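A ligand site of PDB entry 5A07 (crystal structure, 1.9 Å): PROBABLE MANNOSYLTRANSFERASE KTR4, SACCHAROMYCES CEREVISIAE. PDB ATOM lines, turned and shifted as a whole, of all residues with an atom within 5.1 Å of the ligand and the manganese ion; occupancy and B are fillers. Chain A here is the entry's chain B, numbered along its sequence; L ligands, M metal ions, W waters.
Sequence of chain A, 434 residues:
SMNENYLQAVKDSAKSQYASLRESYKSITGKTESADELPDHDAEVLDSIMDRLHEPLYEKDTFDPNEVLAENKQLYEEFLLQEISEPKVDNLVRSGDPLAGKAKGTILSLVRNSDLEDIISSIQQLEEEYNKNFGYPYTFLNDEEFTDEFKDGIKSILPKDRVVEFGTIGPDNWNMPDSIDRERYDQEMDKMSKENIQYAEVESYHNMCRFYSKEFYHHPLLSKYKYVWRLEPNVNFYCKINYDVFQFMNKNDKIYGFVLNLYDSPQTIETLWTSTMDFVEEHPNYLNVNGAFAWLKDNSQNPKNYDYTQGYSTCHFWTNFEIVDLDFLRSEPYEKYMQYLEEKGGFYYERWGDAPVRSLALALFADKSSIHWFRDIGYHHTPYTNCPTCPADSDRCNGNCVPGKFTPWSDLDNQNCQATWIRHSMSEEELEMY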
ATOM      1  N   LEU A 110     -28.738 -24.062  -7.619  1.00  0.00           N
ATOM      2  CA  LEU A 110     -27.553 -24.261  -6.833  1.00  0.00           C
ATOM      3  C   LEU A 110     -27.100 -22.900  -6.467  1.00  0.00           C
ATOM      4  O   LEU A 110     -26.725 -22.124  -7.342  1.00  0.00           O
ATOM      5  CB  LEU A 110     -26.489 -24.923  -7.703  1.00  0.00           C
ATOM      6  CG  LEU A 110     -25.120 -25.104  -7.071  1.00  0.00           C
ATOM      7  CD1 LEU A 110     -25.178 -26.218  -6.023  1.00  0.00           C
ATOM      8  CD2 LEU A 110     -24.013 -25.402  -8.087  1.00  0.00           C
ATOM      9  N   VAL A 111     -27.122 -22.594  -5.149  1.00  0.00           N
ATOM     10  CA  VAL A 111     -26.784 -21.269  -4.689  1.00  0.00           C
ATOM     11  C   VAL A 111     -26.124 -21.296  -3.307  1.00  0.00           C
ATOM     12  O   VAL A 111     -26.258 -22.285  -2.596  1.00  0.00           O
ATOM     13  CB  VAL A 111     -28.027 -20.374  -4.530  1.00  0.00           C
ATOM     14  CG1 VAL A 111     -28.525 -19.918  -5.911  1.00  0.00           C
ATOM     15  CG2 VAL A 111     -29.175 -21.081  -3.886  1.00  0.00           C
ATOM     16  N   ARG A 112     -25.435 -20.190  -3.010  1.00  0.00           N
ATOM     17  CA  ARG A 112     -24.802 -19.992  -1.742  1.00  0.00           C
ATOM     18  C   ARG A 112     -25.745 -19.211  -0.840  1.00  0.00           C
ATOM     19  O   ARG A 112     -26.687 -18.577  -1.289  1.00  0.00           O
ATOM     20  CB  ARG A 112     -23.523 -19.217  -1.927  1.00  0.00           C
ATOM     21  CG  ARG A 112     -22.412 -19.979  -2.636  1.00  0.00           C
ATOM     22  CD  ARG A 112     -21.309 -19.052  -3.160  1.00  0.00           C
ATOM     23  NE  ARG A 112     -21.957 -18.439  -4.332  1.00  0.00           N
ATOM     24  CZ  ARG A 112     -21.395 -18.168  -5.513  1.00  0.00           C
ATOM     25  NH1 ARG A 112     -20.116 -18.413  -5.698  1.00  0.00           N
ATOM     26  NH2 ARG A 112     -22.146 -17.664  -6.500  1.00  0.00           N
ATOM     27  N   ASP A 115     -26.236 -15.742  -1.746  1.00  0.00           N
ATOM     28  CA  ASP A 115     -26.911 -15.384  -3.018  1.00  0.00           C
ATOM     29  C   ASP A 115     -28.341 -15.077  -2.753  1.00  0.00           C
ATOM     30  O   ASP A 115     -29.153 -14.911  -3.680  1.00  0.00           O
ATOM     31  CB  ASP A 115     -26.812 -16.564  -3.982  1.00  0.00           C
ATOM     32  CG  ASP A 115     -25.448 -16.738  -4.534  1.00  0.00           C
ATOM     33  OD1 ASP A 115     -24.823 -15.716  -4.910  1.00  0.00           O
ATOM     34  OD2 ASP A 115     -24.938 -17.875  -4.592  1.00  0.00           O
ATOM     35  N   LEU A 141     -29.983 -26.350  -3.705  1.00  0.00           N
ATOM     36  CA  LEU A 141     -28.825 -27.128  -3.307  1.00  0.00           C
ATOM     37  C   LEU A 141     -27.662 -26.278  -3.044  1.00  0.00           C
ATOM     38  O   LEU A 141     -27.487 -25.256  -3.666  1.00  0.00           O
ATOM     39  CB  LEU A 141     -28.427 -28.159  -4.389  1.00  0.00           C
ATOM     40  CG  LEU A 141     -29.490 -29.148  -4.848  1.00  0.00           C
ATOM     41  CD1 LEU A 141     -29.024 -30.084  -6.021  1.00  0.00           C
ATOM     42  CD2 LEU A 141     -30.012 -29.978  -3.655  1.00  0.00           C
ATOM     43  N   ASN A 142     -26.816 -26.699  -2.076  1.00  0.00           N
ATOM     44  CA  ASN A 142     -25.640 -25.942  -1.707  1.00  0.00           C
ATOM     45  C   ASN A 142     -24.551 -26.917  -1.207  1.00  0.00           C
ATOM     46  O   ASN A 142     -24.889 -27.958  -0.656  1.00  0.00           O
ATOM     47  CB  ASN A 142     -26.106 -24.963  -0.598  1.00  0.00           C
ATOM     48  CG  ASN A 142     -25.050 -23.932  -0.171  1.00  0.00           C
ATOM     49  OD1 ASN A 142     -23.882 -23.904  -0.582  1.00  0.00           O
ATOM     50  ND2 ASN A 142     -25.508 -23.040   0.705  1.00  0.00           N
ATOM     51  N   ASP A 143     -23.294 -26.542  -1.370  1.00  0.00           N
ATOM     52  CA  ASP A 143     -22.195 -27.337  -0.799  1.00  0.00           C
ATOM     53  C   ASP A 143     -22.055 -27.122   0.719  1.00  0.00           C
ATOM     54  O   ASP A 143     -21.416 -27.930   1.367  1.00  0.00           O
ATOM     55  CB  ASP A 143     -20.849 -27.048  -1.487  1.00  0.00           C
ATOM     56  CG  ASP A 143     -20.451 -25.598  -1.429  1.00  0.00           C
ATOM     57  OD1 ASP A 143     -21.223 -24.690  -1.814  1.00  0.00           O
ATOM     58  OD2 ASP A 143     -19.318 -25.296  -1.030  1.00  0.00           O
ATOM     59  N   TRP A 174     -18.881 -33.131  -4.133  1.00  0.00           N
ATOM     60  CA  TRP A 174     -18.575 -31.741  -4.465  1.00  0.00           C
ATOM     61  C   TRP A 174     -17.079 -31.493  -4.612  1.00  0.00           C
ATOM     62  O   TRP A 174     -16.623 -30.953  -5.611  1.00  0.00           O
ATOM     63  CB  TRP A 174     -19.179 -30.809  -3.393  1.00  0.00           C
ATOM     64  CG  TRP A 174     -18.895 -29.375  -3.641  1.00  0.00           C
ATOM     65  CD1 TRP A 174     -17.874 -28.670  -3.130  1.00  0.00           C
ATOM     66  CD2 TRP A 174     -19.578 -28.512  -4.560  1.00  0.00           C
ATOM     67  NE1 TRP A 174     -17.880 -27.427  -3.643  1.00  0.00           N
ATOM     68  CE2 TRP A 174     -18.941 -27.294  -4.497  1.00  0.00           C
ATOM     69  CE3 TRP A 174     -20.705 -28.671  -5.395  1.00  0.00           C
ATOM     70  CZ2 TRP A 174     -19.348 -26.186  -5.249  1.00  0.00           C
ATOM     71  CZ3 TRP A 174     -21.118 -27.597  -6.149  1.00  0.00           C
ATOM     72  CH2 TRP A 174     -20.459 -26.352  -6.059  1.00  0.00           C
ATOM     73  N   TYR A 199     -12.015 -17.150 -13.380  1.00  0.00           N
ATOM     74  CA  TYR A 199     -12.199 -18.160 -12.341  1.00  0.00           C
ATOM     75  C   TYR A 199     -11.170 -19.254 -12.369  1.00  0.00           C
ATOM     76  O   TYR A 199     -11.368 -20.299 -11.752  1.00  0.00           O
ATOM     77  CB  TYR A 199     -13.527 -18.875 -12.461  1.00  0.00           C
ATOM     78  CG  TYR A 199     -14.784 -18.036 -12.499  1.00  0.00           C
ATOM     79  CD1 TYR A 199     -15.179 -17.225 -11.419  1.00  0.00           C
ATOM     80  CD2 TYR A 199     -15.612 -18.112 -13.617  1.00  0.00           C
ATOM     81  CE1 TYR A 199     -16.355 -16.492 -11.474  1.00  0.00           C
ATOM     82  CE2 TYR A 199     -16.792 -17.387 -13.676  1.00  0.00           C
ATOM     83  CZ  TYR A 199     -17.188 -16.602 -12.615  1.00  0.00           C
ATOM     84  OH  TYR A 199     -18.395 -15.929 -12.766  1.00  0.00           O
ATOM     85  N   SER A 204     -13.778 -23.480  -6.071  1.00  0.00           N
ATOM     86  CA  SER A 204     -15.237 -23.731  -5.957  1.00  0.00           C
ATOM     87  C   SER A 204     -15.888 -23.765  -7.399  1.00  0.00           C
ATOM     88  O   SER A 204     -16.897 -24.425  -7.584  1.00  0.00           O
ATOM     89  CB  SER A 204     -15.861 -22.687  -5.099  1.00  0.00           C
ATOM     90  OG  SER A 204     -15.681 -21.416  -5.662  1.00  0.00           O
ATOM     91  N   TYR A 205     -15.324 -22.991  -8.312  1.00  0.00           N
ATOM     92  CA  TYR A 205     -15.906 -22.837  -9.661  1.00  0.00           C
ATOM     93  C   TYR A 205     -15.681 -24.094 -10.442  1.00  0.00           C
ATOM     94  O   TYR A 205     -16.588 -24.603 -11.129  1.00  0.00           O
ATOM     95  CB  TYR A 205     -15.331 -21.622 -10.365  1.00  0.00           C
ATOM     96  CG  TYR A 205     -16.140 -21.313 -11.620  1.00  0.00           C
ATOM     97  CD1 TYR A 205     -17.297 -20.550 -11.529  1.00  0.00           C
ATOM     98  CD2 TYR A 205     -15.764 -21.794 -12.866  1.00  0.00           C
ATOM     99  CE1 TYR A 205     -18.055 -20.245 -12.679  1.00  0.00           C
ATOM    100  CE2 TYR A 205     -16.529 -21.526 -14.031  1.00  0.00           C
ATOM    101  CZ  TYR A 205     -17.663 -20.754 -13.907  1.00  0.00           C
ATOM    102  OH  TYR A 205     -18.437 -20.438 -14.984  1.00  0.00           O
ATOM    103  N   MET A 208     -18.082 -26.520  -9.034  1.00  0.00           N
ATOM    104  CA  MET A 208     -19.434 -26.258  -9.548  1.00  0.00           C
ATOM    105  C   MET A 208     -19.636 -26.819 -10.964  1.00  0.00           C
ATOM    106  O   MET A 208     -20.623 -27.489 -11.255  1.00  0.00           O
ATOM    107  CB  MET A 208     -19.700 -24.797  -9.506  1.00  0.00           C
ATOM    108  CG  MET A 208     -21.098 -24.396 -10.035  1.00  0.00           C
ATOM    109  SD  MET A 208     -21.161 -24.183 -11.844  1.00  0.00           S
ATOM    110  CE  MET A 208     -20.049 -22.839 -12.234  1.00  0.00           C
ATOM    111  N   TYR A 212     -22.374 -29.584 -11.782  1.00  0.00           N
ATOM    112  CA  TYR A 212     -23.510 -29.334 -12.777  1.00  0.00           C
ATOM    113  C   TYR A 212     -23.391 -30.223 -14.016  1.00  0.00           C
ATOM    114  O   TYR A 212     -24.400 -30.502 -14.697  1.00  0.00           O
ATOM    115  CB  TYR A 212     -23.630 -27.838 -13.116  1.00  0.00           C
ATOM    116  CG  TYR A 212     -24.842 -27.172 -12.480  1.00  0.00           C
ATOM    117  CD1 TYR A 212     -26.088 -27.813 -12.484  1.00  0.00           C
ATOM    118  CD2 TYR A 212     -24.767 -25.882 -11.876  1.00  0.00           C
ATOM    119  CE1 TYR A 212     -27.207 -27.207 -11.925  1.00  0.00           C
ATOM    120  CE2 TYR A 212     -25.891 -25.276 -11.362  1.00  0.00           C
ATOM    121  CZ  TYR A 212     -27.104 -25.926 -11.380  1.00  0.00           C
ATOM    122  OH  TYR A 212     -28.273 -25.314 -10.857  1.00  0.00           O
ATOM    123  N   ARG A 230     -33.377 -25.189 -14.505  1.00  0.00           N
ATOM    124  CA  ARG A 230     -32.280 -24.512 -13.836  1.00  0.00           C
ATOM    125  C   ARG A 230     -32.454 -22.990 -13.789  1.00  0.00           C
ATOM    126  O   ARG A 230     -32.585 -22.352 -14.839  1.00  0.00           O
ATOM    127  CB  ARG A 230     -30.972 -24.851 -14.491  1.00  0.00           C
ATOM    128  CG  ARG A 230     -29.746 -24.169 -13.888  1.00  0.00           C
ATOM    129  CD  ARG A 230     -28.561 -24.839 -14.512  1.00  0.00           C
ATOM    130  NE  ARG A 230     -27.344 -24.117 -14.316  1.00  0.00           N
ATOM    131  CZ  ARG A 230     -26.189 -24.532 -14.782  1.00  0.00           C
ATOM    132  NH1 ARG A 230     -26.079 -25.672 -15.433  1.00  0.00           N
ATOM    133  NH2 ARG A 230     -25.119 -23.802 -14.577  1.00  0.00           N
ATOM    134  N   LEU A 231     -32.356 -22.439 -12.574  1.00  0.00           N
ATOM    135  CA  LEU A 231     -32.450 -21.021 -12.292  1.00  0.00           C
ATOM    136  C   LEU A 231     -31.185 -20.547 -11.577  1.00  0.00           C
ATOM    137  O   LEU A 231     -30.700 -21.206 -10.648  1.00  0.00           O
ATOM    138  CB  LEU A 231     -33.638 -20.791 -11.379  1.00  0.00           C
ATOM    139  CG  LEU A 231     -33.963 -19.340 -11.129  1.00  0.00           C
ATOM    140  CD1 LEU A 231     -34.470 -18.643 -12.394  1.00  0.00           C
ATOM    141  CD2 LEU A 231     -35.034 -19.292 -10.059  1.00  0.00           C
ATOM    142  N   GLU A 232     -30.606 -19.447 -12.042  1.00  0.00           N
ATOM    143  CA  GLU A 232     -29.421 -18.870 -11.408  1.00  0.00           C
ATOM    144  C   GLU A 232     -29.757 -17.495 -10.834  1.00  0.00           C
ATOM    145  O   GLU A 232     -30.773 -16.889 -11.196  1.00  0.00           O
ATOM    146  CB  GLU A 232     -28.284 -18.682 -12.404  1.00  0.00           C
ATOM    147  CG  GLU A 232     -27.703 -19.986 -12.876  1.00  0.00           C
ATOM    148  CD  GLU A 232     -26.259 -19.936 -13.343  1.00  0.00           C
ATOM    149  OE1 GLU A 232     -25.669 -18.839 -13.509  1.00  0.00           O
ATOM    150  OE2 GLU A 232     -25.788 -21.026 -13.739  1.00  0.00           O
ATOM    151  N   PRO A 233     -28.943 -17.045  -9.900  1.00  0.00           N
ATOM    152  CA  PRO A 233     -29.191 -15.721  -9.336  1.00  0.00           C
ATOM    153  C   PRO A 233     -29.071 -14.601 -10.384  1.00  0.00           C
ATOM    154  O   PRO A 233     -28.294 -14.724 -11.321  1.00  0.00           O
ATOM    155  CB  PRO A 233     -28.080 -15.555  -8.295  1.00  0.00           C
ATOM    156  CG  PRO A 233     -27.692 -16.927  -7.961  1.00  0.00           C
ATOM    157  CD  PRO A 233     -27.815 -17.686  -9.249  1.00  0.00           C
ATOM    158  N   ASN A 320     -26.861 -21.463 -17.948  1.00  0.00           N
ATOM    159  CA  ASN A 320     -27.460 -20.788 -16.802  1.00  0.00           C
ATOM    160  C   ASN A 320     -28.966 -20.883 -16.786  1.00  0.00           C
ATOM    161  O   ASN A 320     -29.594 -20.798 -15.746  1.00  0.00           O
ATOM    162  CB  ASN A 320     -26.926 -19.371 -16.611  1.00  0.00           C
ATOM    163  CG  ASN A 320     -27.048 -18.481 -17.843  1.00  0.00           C
ATOM    164  OD1 ASN A 320     -28.135 -18.181 -18.280  1.00  0.00           O
ATOM    165  ND2 ASN A 320     -25.936 -18.017 -18.322  1.00  0.00           N
ATOM    166  N   HIS A 381     -29.219 -13.031 -18.755  1.00  0.00           N
ATOM    167  CA  HIS A 381     -28.185 -13.239 -17.768  1.00  0.00           C
ATOM    168  C   HIS A 381     -27.037 -12.471 -18.338  1.00  0.00           C
ATOM    169  O   HIS A 381     -26.642 -12.637 -19.524  1.00  0.00           O
ATOM    170  CB  HIS A 381     -27.837 -14.722 -17.670  1.00  0.00           C
ATOM    171  CG  HIS A 381     -26.704 -15.072 -16.717  1.00  0.00           C
ATOM    172  ND1 HIS A 381     -25.414 -14.637 -16.862  1.00  0.00           N
ATOM    173  CD2 HIS A 381     -26.711 -15.832 -15.597  1.00  0.00           C
ATOM    174  CE1 HIS A 381     -24.659 -15.162 -15.912  1.00  0.00           C
ATOM    175  NE2 HIS A 381     -25.429 -15.881 -15.127  1.00  0.00           N
HETATM  176  P1  LIG L   1     -21.325 -18.028 -14.118  1.00  0.00           P
HETATM  177  O1  LIG L   1     -20.596 -16.741 -14.014  1.00  0.00           O
HETATM  178  O2  LIG L   1     -20.731 -19.106 -14.822  1.00  0.00           O
HETATM  179  O3  LIG L   1     -22.770 -17.825 -14.384  1.00  0.00           O
HETATM  180  O4  LIG L   1     -21.120 -18.602 -12.617  1.00  0.00           O
HETATM  181  P2  LIG L   1     -21.984 -18.450 -11.293  1.00  0.00           P
HETATM  182  O5  LIG L   1     -21.221 -17.952 -10.153  1.00  0.00           O
HETATM  183  O6  LIG L   1     -23.316 -17.834 -11.448  1.00  0.00           O
HETATM  184  O7  LIG L   1     -22.218 -19.980 -10.971  1.00  0.00           O
HETATM  185  C1  LIG L   1     -23.161 -20.890 -11.543  1.00  0.00           C
HETATM  186  C2  LIG L   1     -24.219 -21.353 -10.562  1.00  0.00           C
HETATM  187  O8  LIG L   1     -23.568 -22.102  -9.542  1.00  0.00           O
HETATM  188  C3  LIG L   1     -24.991 -20.231  -9.892  1.00  0.00           C
HETATM  189  O9  LIG L   1     -26.330 -20.709  -9.580  1.00  0.00           O
HETATM  190  C4  LIG L   1     -24.171 -19.985  -8.614  1.00  0.00           C
HETATM  191  O10 LIG L   1     -24.972 -19.483  -7.555  1.00  0.00           O
HETATM  192  C5  LIG L   1     -23.740 -21.368  -8.303  1.00  0.00           C
HETATM  193  N1  LIG L   1     -22.429 -21.456  -7.627  1.00  0.00           N
HETATM  194  C6  LIG L   1     -21.202 -21.088  -8.077  1.00  0.00           C
HETATM  195  N2  LIG L   1     -20.239 -21.411  -7.128  1.00  0.00           N
HETATM  196  C7  LIG L   1     -20.900 -22.016  -6.085  1.00  0.00           C
HETATM  197  C8  LIG L   1     -20.472 -22.599  -4.799  1.00  0.00           C
HETATM  198  O11 LIG L   1     -19.222 -22.547  -4.583  1.00  0.00           O
HETATM  199  N3  LIG L   1     -21.428 -23.090  -3.992  1.00  0.00           N
HETATM  200  C9  LIG L   1     -22.773 -23.053  -4.321  1.00  0.00           C
HETATM  201  N4  LIG L   1     -23.662 -23.559  -3.476  1.00  0.00           N
HETATM  202  N5  LIG L   1     -23.212 -22.524  -5.507  1.00  0.00           N
HETATM  203  C10 LIG L   1     -22.330 -22.064  -6.403  1.00  0.00           C
HETATM  204 MN    MN M   1     -24.469 -17.048 -13.247  1.00  0.00          MN
HETATM  205  O   HOH W   1     -23.226 -15.045 -12.937  1.00  0.00           O
HETATM  206  O   HOH W   2     -25.969 -15.982 -11.723  1.00  0.00           O
HETATM  207  O   HOH W   3     -18.314 -19.848  -4.187  1.00  0.00           O
HETATM  208  O   HOH W   4     -23.246 -18.293 -17.113  1.00  0.00           O
HETATM  209  O   HOH W   5     -17.686 -20.818  -7.524  1.00  0.00           O
HETATM  210  O   HOH W   6     -28.370 -22.671 -10.389  1.00  0.00           O
HETATM  211  O   HOH W   7     -23.578 -20.676 -15.333  1.00  0.00           O
HETATM  212  O   HOH W   8     -17.913 -23.632  -2.398  1.00  0.00           O
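Water W5 lies within hydrogen-bond range of a nitrogen (N2) of the ligand, the side-chain hydroxyl of Ser 204 and the backbone NH of Tyr 205. Water W8 lies within hydrogen-bond range of the side-chain carboxylate of Asp 143 (2.6 Å) and an oxygen (O11) of the ligand (2.8 Å). Water W4 lies within hydrogen-bond range of ND2 of Asn 320 (3.0 Å) and O2 of the ligand (3.5 Å). Water W3 lies within hydrogen-bond range of the guanidinium group (NH1) of Arg 112, an oxygen (O11) of the ligand and the side-chain hydroxyl (OG) of Ser 204. Water W6 lies within hydrogen-bond range of the side-chain hydroxyl of Tyr 212, the backbone carbonyl oxygen of Leu 231, an oxygen (O9) of the ligand and the backbone NH of Leu 110. Water W7 bridges OE2 of Glu 232 and O2 of the ligand.
Within 4 Å of the manganese ion: Glu 232 and His 381. The nearest printed residue that does not touch the manganese ion is Asn 320 (4.8 Å).
The manganese ion is bound by the side-chain carboxylate of Glu 232 (2.2 Å), an oxygen (O3) of the ligand (2.2 Å), an oxygen (O6) of the ligand (2.3 Å), water W1 (2.4 Å), water W2 (2.4 Å) and a ring nitrogen (NE2) of His 381 (2.4 Å).
The guanidinium group (NH2) of Arg 230 lies within salt-bridge range of the side-chain carboxylate (OE2) of Glu 232 (3.0 Å). OD1 of Asp 143 sits close to OD1 of Asn 142, 3.0 Å away. The side-chain amide nitrogen (ND2) of Asn 142 lies close to the backbone carbonyl oxygen (O) of Val 111, 3.5 Å away. N of Val 111 lies within hydrogen-bond range of O of Leu 141. NE of Arg 112 is in salt-bridge range of OD2 of Asp 115.
CZ2 of Trp 174 touches O11 of the ligand, at 3.7 Å. Ser 204 touches the ligand (CB to O11, 3.4 Å). CG of Met 208 touches O8 of the ligand, at 3.4 Å. Pro 233 touches the ligand. Hydrophobic or aromatic side chains within 4 Å of the ligand: Leu 110, Val 111, Trp 174, Tyr 199, Tyr 205, Met 208, Pro 233 and His 381. 14 residues have an atom within 4 Å of the ligand: Leu 110, Val 111, Arg 112, Asp 115, Asn 142, Asp 143, Trp 174, Tyr 199, Ser 204, Tyr 205, Met 208, Glu 232, Pro 233 and His 381. The nearest printed residue that does not touch the ligand is Leu 141 (4.2 Å).
O1 of the ligand lies within hydrogen-bond range of OH of Tyr 199, 2.7 Å away. The side-chain hydroxyl (OH) of Tyr 205 is in hydrogen-bond range of an oxygen (O2) of the ligand, 2.7 Å away. The backbone carbonyl oxygen (O) of Leu 110 is in hydrogen-bond range of an oxygen (O9) of the ligand (2.7 Å). A nitrogen (N3) of the ligand is in hydrogen-bond range of the side-chain carboxylate (OD1) of Asp 143. A nitrogen (N4) of the ligand lies within hydrogen-bond range of the side-chain amide oxygen (OD1) of Asn 142 (2.9 Å). O of Val 111 is in hydrogen-bond range of N4 of the ligand, at 3.0 Å. The guanidinium group of Arg 112 is in salt-bridge range of an oxygen (O5) of the ligand, at 3.8 Å. O10 of the ligand sits at hydrogen-bond distance from OD2 of Asp 115, at 3.4 Å.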
